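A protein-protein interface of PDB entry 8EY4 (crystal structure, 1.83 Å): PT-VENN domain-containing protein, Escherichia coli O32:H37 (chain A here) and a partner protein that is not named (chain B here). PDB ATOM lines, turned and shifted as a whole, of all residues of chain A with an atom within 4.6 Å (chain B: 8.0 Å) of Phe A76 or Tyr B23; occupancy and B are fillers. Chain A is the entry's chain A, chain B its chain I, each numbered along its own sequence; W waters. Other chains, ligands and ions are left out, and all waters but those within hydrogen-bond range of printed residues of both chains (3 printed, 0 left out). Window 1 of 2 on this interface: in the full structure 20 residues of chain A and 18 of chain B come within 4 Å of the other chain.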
ATOM      1  N   HIS A  11     -18.836  12.118  16.913  1.00  0.00           N
ATOM      2  CA  HIS A  11     -17.638  11.838  16.124  1.00  0.00           C
ATOM      3  C   HIS A  11     -16.833  13.107  15.860  1.00  0.00           C
ATOM      4  O   HIS A  11     -15.602  13.077  15.904  1.00  0.00           O
ATOM      5  CB  HIS A  11     -18.033  11.108  14.827  1.00  0.00           C
ATOM      6  CG  HIS A  11     -18.262   9.648  15.042  1.00  0.00           C
ATOM      7  ND1 HIS A  11     -19.478   9.137  15.447  1.00  0.00           N
ATOM      8  CD2 HIS A  11     -17.395   8.602  15.043  1.00  0.00           C
ATOM      9  CE1 HIS A  11     -19.370   7.837  15.633  1.00  0.00           C
ATOM     10  NE2 HIS A  11     -18.114   7.485  15.404  1.00  0.00           N
ATOM     11  N   HIS A  15     -12.978  13.366  16.842  1.00  0.00           N
ATOM     12  CA  HIS A  15     -12.014  13.353  15.752  1.00  0.00           C
ATOM     13  C   HIS A  15     -11.757  14.720  15.135  1.00  0.00           C
ATOM     14  O   HIS A  15     -10.960  14.822  14.187  1.00  0.00           O
ATOM     15  CB  HIS A  15     -12.510  12.397  14.668  1.00  0.00           C
ATOM     16  CG  HIS A  15     -12.571  10.990  15.138  1.00  0.00           C
ATOM     17  ND1 HIS A  15     -11.466  10.347  15.651  1.00  0.00           N
ATOM     18  CD2 HIS A  15     -13.596  10.110  15.206  1.00  0.00           C
ATOM     19  CE1 HIS A  15     -11.810   9.117  16.008  1.00  0.00           C
ATOM     20  NE2 HIS A  15     -13.097   8.950  15.741  1.00  0.00           N
ATOM     21  N   GLU A  18      -8.285  16.077  14.279  1.00  0.00           N
ATOM     22  CA  GLU A  18      -7.631  15.484  13.114  1.00  0.00           C
ATOM     23  C   GLU A  18      -7.955  16.200  11.811  1.00  0.00           C
ATOM     24  O   GLU A  18      -7.330  15.899  10.784  1.00  0.00           O
ATOM     25  CB  GLU A  18      -8.028  14.014  12.978  1.00  0.00           C
ATOM     26  CG  GLU A  18      -7.686  13.156  14.181  1.00  0.00           C
ATOM     27  CD  GLU A  18      -8.634  11.980  14.382  1.00  0.00           C
ATOM     28  OE1 GLU A  18      -9.086  11.385  13.381  1.00  0.00           O
ATOM     29  OE2 GLU A  18      -8.922  11.637  15.558  1.00  0.00           O
ATOM     30  N   PHE A  19      -8.903  17.132  11.818  1.00  0.00           N
ATOM     31  CA  PHE A  19      -9.368  17.778  10.590  1.00  0.00           C
ATOM     32  C   PHE A  19      -9.510  19.269  10.846  1.00  0.00           C
ATOM     33  O   PHE A  19     -10.619  19.806  10.831  1.00  0.00           O
ATOM     34  CB  PHE A  19     -10.710  17.205  10.134  1.00  0.00           C
ATOM     35  CG  PHE A  19     -10.687  15.745   9.814  1.00  0.00           C
ATOM     36  CD1 PHE A  19     -10.408  15.306   8.523  1.00  0.00           C
ATOM     37  CD2 PHE A  19     -10.987  14.807  10.795  1.00  0.00           C
ATOM     38  CE1 PHE A  19     -10.414  13.963   8.228  1.00  0.00           C
ATOM     39  CE2 PHE A  19     -10.983  13.451  10.505  1.00  0.00           C
ATOM     40  CZ  PHE A  19     -10.685  13.028   9.231  1.00  0.00           C
ATOM     41  N   ASN A  61      -4.324   9.438   4.793  1.00  0.00           N
ATOM     42  CA  ASN A  61      -4.542   8.663   6.022  1.00  0.00           C
ATOM     43  C   ASN A  61      -5.973   8.780   6.526  1.00  0.00           C
ATOM     44  O   ASN A  61      -6.210   8.774   7.737  1.00  0.00           O
ATOM     45  CB  ASN A  61      -3.567   9.055   7.142  1.00  0.00           C
ATOM     46  CG  ASN A  61      -3.582   8.040   8.281  1.00  0.00           C
ATOM     47  OD1 ASN A  61      -3.837   6.855   8.046  1.00  0.00           O
ATOM     48  ND2 ASN A  61      -3.368   8.504   9.512  1.00  0.00           N
ATOM     49  N   VAL A  62      -6.945   8.910   5.636  1.00  0.00           N
ATOM     50  CA  VAL A  62      -8.336   9.093   6.047  1.00  0.00           C
ATOM     51  C   VAL A  62      -9.086   7.781   5.932  1.00  0.00           C
ATOM     52  O   VAL A  62      -9.153   7.189   4.852  1.00  0.00           O
ATOM     53  CB  VAL A  62      -9.032  10.179   5.228  1.00  0.00           C
ATOM     54  CG1 VAL A  62     -10.505  10.187   5.593  1.00  0.00           C
ATOM     55  CG2 VAL A  62      -8.410  11.506   5.525  1.00  0.00           C
ATOM     56  N   PHE A  63      -9.646   7.318   7.055  1.00  0.00           N
ATOM     57  CA  PHE A  63     -10.545   6.176   7.080  1.00  0.00           C
ATOM     58  C   PHE A  63     -11.985   6.662   7.284  1.00  0.00           C
ATOM     59  O   PHE A  63     -12.232   7.569   8.096  1.00  0.00           O
ATOM     60  CB  PHE A  63     -10.168   5.245   8.231  1.00  0.00           C
ATOM     61  CG  PHE A  63     -11.051   4.042   8.343  1.00  0.00           C
ATOM     62  CD1 PHE A  63     -10.705   2.864   7.701  1.00  0.00           C
ATOM     63  CD2 PHE A  63     -12.198   4.067   9.136  1.00  0.00           C
ATOM     64  CE1 PHE A  63     -11.519   1.730   7.803  1.00  0.00           C
ATOM     65  CE2 PHE A  63     -13.017   2.950   9.261  1.00  0.00           C
ATOM     66  CZ  PHE A  63     -12.687   1.778   8.574  1.00  0.00           C
ATOM     67  N   SER A  65     -16.411   5.083   7.089  1.00  0.00           N
ATOM     68  CA  SER A  65     -17.320   3.984   6.811  1.00  0.00           C
ATOM     69  C   SER A  65     -18.741   4.516   6.746  1.00  0.00           C
ATOM     70  O   SER A  65     -19.069   5.551   7.342  1.00  0.00           O
ATOM     71  CB  SER A  65     -17.185   2.853   7.855  1.00  0.00           C
ATOM     72  OG  SER A  65     -18.218   1.879   7.735  1.00  0.00           O
ATOM     73  N   ARG A  73     -20.868   6.274   9.246  1.00  0.00           N
ATOM     74  CA  ARG A  73     -20.629   5.777  10.605  1.00  0.00           C
ATOM     75  C   ARG A  73     -19.556   6.585  11.313  1.00  0.00           C
ATOM     76  O   ARG A  73     -19.727   6.944  12.484  1.00  0.00           O
ATOM     77  CB  ARG A  73     -20.178   4.308  10.605  1.00  0.00           C
ATOM     78  CG  ARG A  73     -21.078   3.338   9.900  1.00  0.00           C
ATOM     79  CD  ARG A  73     -22.072   2.735  10.823  1.00  0.00           C
ATOM     80  NE  ARG A  73     -22.629   1.526  10.226  1.00  0.00           N
ATOM     81  CZ  ARG A  73     -23.782   0.999  10.606  1.00  0.00           C
ATOM     82  NH1 ARG A  73     -24.469   1.581  11.571  1.00  0.00           N
ATOM     83  NH2 ARG A  73     -24.247  -0.092  10.017  1.00  0.00           N
ATOM     84  N   THR A  74     -18.434   6.848  10.626  1.00  0.00           N
ATOM     85  CA  THR A  74     -17.281   7.472  11.254  1.00  0.00           C
ATOM     86  C   THR A  74     -16.348   8.016  10.176  1.00  0.00           C
ATOM     87  O   THR A  74     -16.422   7.628   9.009  1.00  0.00           O
ATOM     88  CB  THR A  74     -16.537   6.470  12.154  1.00  0.00           C
ATOM     89  OG1 THR A  74     -15.539   7.152  12.903  1.00  0.00           O
ATOM     90  CG2 THR A  74     -15.840   5.404  11.300  1.00  0.00           C
ATOM     91  N   MET A  75     -15.499   8.954  10.581  1.00  0.00           N
ATOM     92  CA  MET A  75     -14.340   9.328   9.750  1.00  0.00           C
ATOM     93  C   MET A  75     -13.226   9.773  10.672  1.00  0.00           C
ATOM     94  O   MET A  75     -13.465  10.568  11.612  1.00  0.00           O
ATOM     95  CB  MET A  75     -14.660  10.448   8.723  1.00  0.00           C
ATOM     96  CG  MET A  75     -13.390  10.936   8.066  1.00  0.00           C
ATOM     97  SD  MET A  75     -13.779  12.168   6.550  1.00  0.00           S
ATOM     98  CE  MET A  75     -14.198  13.791   7.657  1.00  0.00           C
ATOM     99  N   PHE A  76     -12.029   9.224  10.465  1.00  0.00           N
ATOM    100  CA  PHE A  76     -10.902   9.530  11.337  1.00  0.00           C
ATOM    101  C   PHE A  76      -9.607   9.202  10.608  1.00  0.00           C
ATOM    102  O   PHE A  76      -9.597   8.529   9.573  1.00  0.00           O
ATOM    103  CB  PHE A  76     -10.961   8.766  12.677  1.00  0.00           C
ATOM    104  CG  PHE A  76     -11.025   7.257  12.537  1.00  0.00           C
ATOM    105  CD1 PHE A  76      -9.844   6.498  12.440  1.00  0.00           C
ATOM    106  CD2 PHE A  76     -12.260   6.598  12.589  1.00  0.00           C
ATOM    107  CE1 PHE A  76      -9.883   5.116  12.332  1.00  0.00           C
ATOM    108  CE2 PHE A  76     -12.332   5.206  12.480  1.00  0.00           C
ATOM    109  CZ  PHE A  76     -11.143   4.452  12.361  1.00  0.00           C
ATOM    110  N   LYS A  77      -8.511   9.631  11.215  1.00  0.00           N
ATOM    111  CA  LYS A  77      -7.161   9.356  10.746  1.00  0.00           C
ATOM    112  C   LYS A  77      -6.482   8.418  11.732  1.00  0.00           C
ATOM    113  O   LYS A  77      -6.016   8.871  12.789  1.00  0.00           O
ATOM    114  CB  LYS A  77      -6.404  10.678  10.627  1.00  0.00           C
ATOM    115  CG  LYS A  77      -7.070  11.611   9.595  1.00  0.00           C
ATOM    116  CD  LYS A  77      -6.272  12.890   9.373  1.00  0.00           C
ATOM    117  CE  LYS A  77      -6.950  13.815   8.360  1.00  0.00           C
ATOM    118  NZ  LYS A  77      -6.139  15.066   8.164  1.00  0.00           N
ATOM    119  N   PRO A  78      -6.395   7.112  11.442  1.00  0.00           N
ATOM    120  CA  PRO A  78      -5.813   6.162  12.407  1.00  0.00           C
ATOM    121  C   PRO A  78      -4.333   6.414  12.594  1.00  0.00           C
ATOM    122  O   PRO A  78      -3.587   6.542  11.619  1.00  0.00           O
ATOM    123  CB  PRO A  78      -6.045   4.798  11.751  1.00  0.00           C
ATOM    124  CG  PRO A  78      -6.051   5.106  10.288  1.00  0.00           C
ATOM    125  CD  PRO A  78      -6.762   6.449  10.178  1.00  0.00           C
ATOM    126  N   TYR A  84      -3.573  -0.336  10.166  1.00  0.00           N
ATOM    127  CA  TYR A  84      -4.976  -0.428  10.562  1.00  0.00           C
ATOM    128  C   TYR A  84      -5.831  -0.985   9.428  1.00  0.00           C
ATOM    129  O   TYR A  84      -6.663  -1.868   9.633  1.00  0.00           O
ATOM    130  CB  TYR A  84      -5.470   0.955  10.971  1.00  0.00           C
ATOM    131  CG  TYR A  84      -6.934   0.980  11.378  1.00  0.00           C
ATOM    132  CD1 TYR A  84      -7.343   0.380  12.560  1.00  0.00           C
ATOM    133  CD2 TYR A  84      -7.896   1.553  10.547  1.00  0.00           C
ATOM    134  CE1 TYR A  84      -8.680   0.374  12.925  1.00  0.00           C
ATOM    135  CE2 TYR A  84      -9.252   1.565  10.912  1.00  0.00           C
ATOM    136  CZ  TYR A  84      -9.631   0.965  12.103  1.00  0.00           C
ATOM    137  OH  TYR A  84     -10.951   0.962  12.495  1.00  0.00           O
ATOM    138  N   GLN A  88      -8.151  -5.373   8.726  1.00  0.00           N
ATOM    139  CA  GLN A  88      -9.498  -5.870   8.495  1.00  0.00           C
ATOM    140  C   GLN A  88      -9.676  -6.409   7.089  1.00  0.00           C
ATOM    141  O   GLN A  88      -8.732  -6.430   6.294  1.00  0.00           O
ATOM    142  CB  GLN A  88     -10.508  -4.783   8.748  1.00  0.00           C
ATOM    143  CG  GLN A  88     -10.144  -3.512   8.054  1.00  0.00           C
ATOM    144  CD  GLN A  88     -10.573  -2.342   8.883  1.00  0.00           C
ATOM    145  OE1 GLN A  88     -11.687  -2.320   9.391  1.00  0.00           O
ATOM    146  NE2 GLN A  88      -9.671  -1.380   9.072  1.00  0.00           N
ATOM    147  OXT GLN A  88     -10.787  -6.824   6.751  1.00  0.00           O
ATOM    148  N   ILE B  17     -24.678  -0.060  23.201  1.00  0.00           N
ATOM    149  CA  ILE B  17     -24.345  -0.145  21.783  1.00  0.00           C
ATOM    150  C   ILE B  17     -25.565  -0.666  21.045  1.00  0.00           C
ATOM    151  O   ILE B  17     -26.230  -1.609  21.505  1.00  0.00           O
ATOM    152  CB  ILE B  17     -23.117  -1.046  21.558  1.00  0.00           C
ATOM    153  CG1 ILE B  17     -21.860  -0.415  22.183  1.00  0.00           C
ATOM    154  CG2 ILE B  17     -22.890  -1.284  20.067  1.00  0.00           C
ATOM    155  CD1 ILE B  17     -21.659   1.080  21.772  1.00  0.00           C
ATOM    156  N   GLU B  19     -25.606  -1.147  17.260  1.00  0.00           N
ATOM    157  CA  GLU B  19     -25.080  -2.075  16.259  1.00  0.00           C
ATOM    158  C   GLU B  19     -23.637  -2.361  16.620  1.00  0.00           C
ATOM    159  O   GLU B  19     -22.796  -1.448  16.542  1.00  0.00           O
ATOM    160  CB  GLU B  19     -25.153  -1.488  14.846  1.00  0.00           C
ATOM    161  CG  GLU B  19     -26.520  -1.068  14.418  1.00  0.00           C
ATOM    162  CD  GLU B  19     -26.513  -0.479  13.021  1.00  0.00           C
ATOM    163  OE1 GLU B  19     -26.403  -1.278  12.054  1.00  0.00           O
ATOM    164  OE2 GLU B  19     -26.597   0.771  12.902  1.00  0.00           O
ATOM    165  N   PRO B  20     -23.284  -3.577  17.004  1.00  0.00           N
ATOM    166  CA  PRO B  20     -21.916  -3.829  17.460  1.00  0.00           C
ATOM    167  C   PRO B  20     -20.906  -3.695  16.332  1.00  0.00           C
ATOM    168  O   PRO B  20     -21.147  -4.112  15.196  1.00  0.00           O
ATOM    169  CB  PRO B  20     -21.971  -5.269  17.981  1.00  0.00           C
ATOM    170  CG  PRO B  20     -23.142  -5.878  17.303  1.00  0.00           C
ATOM    171  CD  PRO B  20     -24.137  -4.767  17.138  1.00  0.00           C
ATOM    172  N   GLY B  21     -19.746  -3.150  16.668  1.00  0.00           N
ATOM    173  CA  GLY B  21     -18.673  -3.088  15.693  1.00  0.00           C
ATOM    174  C   GLY B  21     -18.877  -2.071  14.590  1.00  0.00           C
ATOM    175  O   GLY B  21     -18.254  -2.187  13.524  1.00  0.00           O
ATOM    176  N   CYS B  22     -19.694  -1.050  14.833  1.00  0.00           N
ATOM    177  CA  CYS B  22     -20.058  -0.055  13.819  1.00  0.00           C
ATOM    178  C   CYS B  22     -19.679   1.352  14.271  1.00  0.00           C
ATOM    179  O   CYS B  22     -20.333   2.328  13.898  1.00  0.00           O
ATOM    180  CB  CYS B  22     -21.551  -0.127  13.500  1.00  0.00           C
ATOM    181  SG  CYS B  22     -22.053  -1.621  12.672  1.00  0.00           S
ATOM    182  N   TYR B  23     -18.633   1.465  15.094  1.00  0.00           N
ATOM    183  CA  TYR B  23     -18.016   2.753  15.457  1.00  0.00           C
ATOM    184  C   TYR B  23     -18.943   3.690  16.233  1.00  0.00           C
ATOM    185  O   TYR B  23     -18.682   4.900  16.313  1.00  0.00           O
ATOM    186  CB  TYR B  23     -17.465   3.468  14.213  1.00  0.00           C
ATOM    187  CG  TYR B  23     -16.409   2.649  13.483  1.00  0.00           C
ATOM    188  CD1 TYR B  23     -15.086   2.647  13.914  1.00  0.00           C
ATOM    189  CD2 TYR B  23     -16.735   1.875  12.376  1.00  0.00           C
ATOM    190  CE1 TYR B  23     -14.094   1.886  13.238  1.00  0.00           C
ATOM    191  CE2 TYR B  23     -15.749   1.125  11.693  1.00  0.00           C
ATOM    192  CZ  TYR B  23     -14.448   1.140  12.141  1.00  0.00           C
ATOM    193  OH  TYR B  23     -13.471   0.405  11.507  1.00  0.00           O
ATOM    194  N   GLU B  24     -19.980   3.174  16.890  1.00  0.00           N
ATOM    195  CA  GLU B  24     -20.697   3.999  17.853  1.00  0.00           C
ATOM    196  C   GLU B  24     -19.768   4.409  18.988  1.00  0.00           C
ATOM    197  O   GLU B  24     -18.888   3.645  19.402  1.00  0.00           O
ATOM    198  CB  GLU B  24     -21.901   3.236  18.404  1.00  0.00           C
ATOM    199  CG  GLU B  24     -22.874   2.846  17.330  1.00  0.00           C
ATOM    200  CD  GLU B  24     -24.000   1.984  17.863  1.00  0.00           C
ATOM    201  OE1 GLU B  24     -24.173   1.935  19.108  1.00  0.00           O
ATOM    202  OE2 GLU B  24     -24.679   1.347  17.033  1.00  0.00           O
ATOM    203  N   ILE B  25     -19.976   5.614  19.518  1.00  0.00           N
ATOM    204  CA  ILE B  25     -19.189   6.101  20.645  1.00  0.00           C
ATOM    205  C   ILE B  25     -20.008   5.910  21.917  1.00  0.00           C
ATOM    206  O   ILE B  25     -21.124   6.425  22.031  1.00  0.00           O
ATOM    207  CB  ILE B  25     -18.762   7.561  20.461  1.00  0.00           C
ATOM    208  CG1 ILE B  25     -17.866   7.694  19.203  1.00  0.00           C
ATOM    209  CG2 ILE B  25     -18.032   8.057  21.692  1.00  0.00           C
ATOM    210  CD1 ILE B  25     -17.547   9.162  18.858  1.00  0.00           C
ATOM    211  N   CYS B  26     -19.470   5.114  22.833  1.00  0.00           N
ATOM    212  CA  CYS B  26     -20.155   4.835  24.097  1.00  0.00           C
ATOM    213  C   CYS B  26     -20.333   6.137  24.865  1.00  0.00           C
ATOM    214  O   CYS B  26     -19.345   6.837  25.120  1.00  0.00           O
ATOM    215  CB  CYS B  26     -19.340   3.850  24.931  1.00  0.00           C
ATOM    216  SG  CYS B  26     -20.173   3.478  26.520  1.00  0.00           S
ATOM    217  N   TRP B  31     -15.455   5.163  24.559  1.00  0.00           N
ATOM    218  CA  TRP B  31     -14.830   4.218  23.630  1.00  0.00           C
ATOM    219  C   TRP B  31     -15.609   4.162  22.325  1.00  0.00           C
ATOM    220  O   TRP B  31     -16.823   3.932  22.348  1.00  0.00           O
ATOM    221  CB  TRP B  31     -14.786   2.820  24.267  1.00  0.00           C
ATOM    222  CG  TRP B  31     -14.170   1.788  23.343  1.00  0.00           C
ATOM    223  CD1 TRP B  31     -14.818   0.821  22.635  1.00  0.00           C
ATOM    224  CD2 TRP B  31     -12.771   1.619  23.073  1.00  0.00           C
ATOM    225  NE1 TRP B  31     -13.899   0.052  21.928  1.00  0.00           N
ATOM    226  CE2 TRP B  31     -12.641   0.539  22.174  1.00  0.00           C
ATOM    227  CE3 TRP B  31     -11.615   2.285  23.499  1.00  0.00           C
ATOM    228  CZ2 TRP B  31     -11.390   0.112  21.682  1.00  0.00           C
ATOM    229  CZ3 TRP B  31     -10.371   1.854  23.010  1.00  0.00           C
ATOM    230  CH2 TRP B  31     -10.280   0.783  22.127  1.00  0.00           C
ATOM    231  N   GLU B  32     -14.917   4.385  21.185  1.00  0.00           N
ATOM    232  CA  GLU B  32     -15.538   4.205  19.876  1.00  0.00           C
ATOM    233  C   GLU B  32     -15.465   2.734  19.490  1.00  0.00           C
ATOM    234  O   GLU B  32     -14.396   2.112  19.570  1.00  0.00           O
ATOM    235  CB  GLU B  32     -14.858   5.069  18.810  1.00  0.00           C
ATOM    236  CG  GLU B  32     -15.533   4.917  17.474  1.00  0.00           C
ATOM    237  CD  GLU B  32     -15.108   5.995  16.489  1.00  0.00           C
ATOM    238  OE1 GLU B  32     -14.355   6.890  16.913  1.00  0.00           O
ATOM    239  OE2 GLU B  32     -15.556   5.943  15.319  1.00  0.00           O
ATOM    240  N   ASP B  33     -16.612   2.158  19.130  1.00  0.00           N
ATOM    241  CA  ASP B  33     -16.722   0.704  19.034  1.00  0.00           C
ATOM    242  C   ASP B  33     -16.148   0.231  17.687  1.00  0.00           C
ATOM    243  O   ASP B  33     -16.845  -0.163  16.755  1.00  0.00           O
ATOM    244  CB  ASP B  33     -18.171   0.279  19.274  1.00  0.00           C
ATOM    245  CG  ASP B  33     -18.367  -1.218  19.168  1.00  0.00           C
ATOM    246  OD1 ASP B  33     -17.363  -1.951  19.252  1.00  0.00           O
ATOM    247  OD2 ASP B  33     -19.525  -1.657  18.993  1.00  0.00           O
ATOM    248  N   ASP B  34     -14.821   0.179  17.658  1.00  0.00           N
ATOM    249  CA  ASP B  34     -14.006  -0.191  16.499  1.00  0.00           C
ATOM    250  C   ASP B  34     -13.780  -1.700  16.480  1.00  0.00           C
ATOM    251  O   ASP B  34     -13.195  -2.237  17.433  1.00  0.00           O
ATOM    252  CB  ASP B  34     -12.683   0.545  16.612  1.00  0.00           C
ATOM    253  CG  ASP B  34     -11.680   0.219  15.489  1.00  0.00           C
ATOM    254  OD1 ASP B  34     -11.572  -0.933  15.056  1.00  0.00           O
ATOM    255  OD2 ASP B  34     -10.945   1.134  15.086  1.00  0.00           O
ATOM    256  N   PRO B  35     -14.173  -2.414  15.421  1.00  0.00           N
ATOM    257  CA  PRO B  35     -14.110  -3.880  15.473  1.00  0.00           C
ATOM    258  C   PRO B  35     -12.686  -4.419  15.363  1.00  0.00           C
ATOM    259  O   PRO B  35     -12.410  -5.521  15.858  1.00  0.00           O
ATOM    260  CB  PRO B  35     -14.982  -4.308  14.282  1.00  0.00           C
ATOM    261  CG  PRO B  35     -14.815  -3.173  13.297  1.00  0.00           C
ATOM    262  CD  PRO B  35     -14.696  -1.919  14.130  1.00  0.00           C
ATOM    263  N   VAL B  36     -11.769  -3.676  14.739  1.00  0.00           N
ATOM    264  CA  VAL B  36     -10.364  -4.095  14.739  1.00  0.00           C
ATOM    265  C   VAL B  36      -9.818  -4.108  16.163  1.00  0.00           C
ATOM    266  O   VAL B  36      -9.080  -5.023  16.557  1.00  0.00           O
ATOM    267  CB  VAL B  36      -9.547  -3.166  13.827  1.00  0.00           C
ATOM    268  CG1 VAL B  36      -8.048  -3.449  13.934  1.00  0.00           C
ATOM    269  CG2 VAL B  36     -10.011  -3.358  12.406  1.00  0.00           C
ATOM    270  N   GLN B  37     -10.180  -3.095  16.956  1.00  0.00           N
ATOM    271  CA  GLN B  37      -9.644  -2.962  18.307  1.00  0.00           C
ATOM    272  C   GLN B  37     -10.335  -3.880  19.312  1.00  0.00           C
ATOM    273  O   GLN B  37      -9.714  -4.233  20.321  1.00  0.00           O
ATOM    274  CB  GLN B  37      -9.725  -1.503  18.760  1.00  0.00           C
ATOM    275  CG  GLN B  37      -8.727  -0.631  17.983  1.00  0.00           C
ATOM    276  CD  GLN B  37      -8.652   0.799  18.492  1.00  0.00           C
ATOM    277  OE1 GLN B  37      -9.579   1.571  18.288  1.00  0.00           O
ATOM    278  NE2 GLN B  37      -7.533   1.169  19.125  1.00  0.00           N
ATOM    279  N   GLY B  45      -4.362   2.799  18.324  1.00  0.00           N
ATOM    280  CA  GLY B  45      -4.192   3.579  17.106  1.00  0.00           C
ATOM    281  C   GLY B  45      -5.140   3.222  15.985  1.00  0.00           C
ATOM    282  O   GLY B  45      -4.776   3.351  14.799  1.00  0.00           O
ATOM    283  N   GLY B  46      -6.370   2.823  16.315  1.00  0.00           N
ATOM    284  CA  GLY B  46      -7.405   2.685  15.309  1.00  0.00           C
ATOM    285  C   GLY B  46      -8.367   3.852  15.486  1.00  0.00           C
ATOM    286  O   GLY B  46      -7.906   4.993  15.537  1.00  0.00           O
ATOM    287  N   ALA B  47      -9.676   3.602  15.628  1.00  0.00           N
ATOM    288  CA  ALA B  47     -10.578   4.723  15.875  1.00  0.00           C
ATOM    289  C   ALA B  47     -10.255   5.389  17.201  1.00  0.00           C
ATOM    290  O   ALA B  47     -10.430   6.598  17.343  1.00  0.00           O
ATOM    291  CB  ALA B  47     -12.042   4.286  15.847  1.00  0.00           C
ATOM    292  N   ASN B  48      -9.737   4.617  18.160  1.00  0.00           N
ATOM    293  CA  ASN B  48      -9.284   5.117  19.455  1.00  0.00           C
ATOM    294  C   ASN B  48      -7.770   5.133  19.515  1.00  0.00           C
ATOM    295  O   ASN B  48      -7.113   4.203  19.037  1.00  0.00           O
ATOM    296  CB  ASN B  48      -9.788   4.240  20.582  1.00  0.00           C
ATOM    297  CG  ASN B  48     -11.303   4.053  20.527  1.00  0.00           C
ATOM    298  OD1 ASN B  48     -12.055   4.916  20.967  1.00  0.00           O
ATOM    299  ND2 ASN B  48     -11.742   2.950  19.975  1.00  0.00           N
HETATM  300  O   HOH W   1      -7.953   8.991  17.053  1.00  0.00           O
HETATM  301  O   HOH W   2     -21.498   4.946  14.007  1.00  0.00           O
HETATM  302  O   HOH W   3     -14.495  -2.018  10.327  1.00  0.00           O
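OE2 of Glu B19 is in salt-bridge range of NH1 of Arg A73. NH2 of Arg A73 lies close to SG of Cys B22. The backbone carbonyl oxygen of Tyr B23 is in hydrogen-bond range of a ring nitrogen (NE2) of His A11, at 2.8 Å. OH of Tyr B23 sits at hydrogen-bond distance from OH of Tyr A84. OE2 of Glu B32 lies within hydrogen-bond range of NE2 of His A11 (3.0 Å). OE1 of Glu B32 sits at hydrogen-bond distance from NE2 of His A15. OE2 of Glu B32 lies within hydrogen-bond range of OG1 of Thr A74. The side-chain hydroxyl (OH) of Tyr A84 sits at hydrogen-bond distance from the side-chain carboxylate (OD2) of Asp B34.
The side-chain carboxylate (OE2) of Glu B24 sits at hydrogen-bond distance from the backbone NH (N) of Glu B19, at 2.7 Å. The backbone carbonyl oxygen of Asp B33 sits at hydrogen-bond distance from the backbone NH of Tyr B23 (2.9 Å). The side-chain amide nitrogen (ND2) of Asn B48 lies within hydrogen-bond range of the backbone carbonyl oxygen (O) of Glu B32 (2.8 Å). O of Arg A73 lies close to NE2 of His A11, at 3.4 Å. A ring nitrogen (ND1) of His A15 is in hydrogen-bond range of the side-chain carboxylate (OE2) of Glu A18, at 2.9 Å. The backbone carbonyl oxygen (O) of Tyr A84 is in hydrogen-bond range of the side-chain amide nitrogen (NE2) of Gln A88 (3.1 Å).
Among the printed residues, merely in contact across the chains: His A15 with Ala B47 (3.2 Å), Phe A63 with Tyr B23 (3.3 Å), Phe A76 with Ala B47 (3.5 Å), Tyr A84 with Gly B46 (3.6 Å), Thr A74 with Tyr B23 (3.6 Å), Gln A88 with Val B36 (3.6 Å), Pro A78 with Gly B45 (3.6 Å), Phe A76 with Gly B46 (3.7 Å), Tyr A84 with Val B36 (3.8 Å), His A11 with Ile B25 (3.8 Å), Phe A76 with Tyr B23 (3.8 Å), Gln A88 with Tyr B23 (3.9 Å) and Pro A78 with Gly B46 (3.9 Å).
Printed residues of chain B within 4 Å of Phe A76: Tyr B23, Gly B46 and Ala B47. Printed residues of chain A within 4 Å of Tyr B23: His A11, Phe A63, Thr A74, Phe A76, Tyr A84 and Gln A88. Printed residues of chain A within 4 Å of Ala B47: His A15 and Phe A76. Of the printed residues of chain B, Pro A78 touches Gly B45 and Gly B46.
Hydrophobic or aromatic side chains of chain B within 4 Å of the printed part of chain A: Tyr B23, Ile B25, Val B36 and Ala B47. Among the printed residues, Asp or Glu carboxylates within 4 Å of a Lys or Arg side-chain nitrogen of the other chain: Arg A73 with Glu B19 (2.6 Å).
Water W2 lies within hydrogen-bond range of O of Cys B22 and O of Arg A73. Water W3 bridges the side-chain hydroxyl (OH) of Tyr B23 (2.9 Å) and the side-chain amide oxygen (OE1) of Gln A88 (3.0 Å). Water W1 bridges the side-chain carboxylate of Glu A18 (3.2 Å) and the backbone carbonyl oxygen of Ala B47 (3.5 Å).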
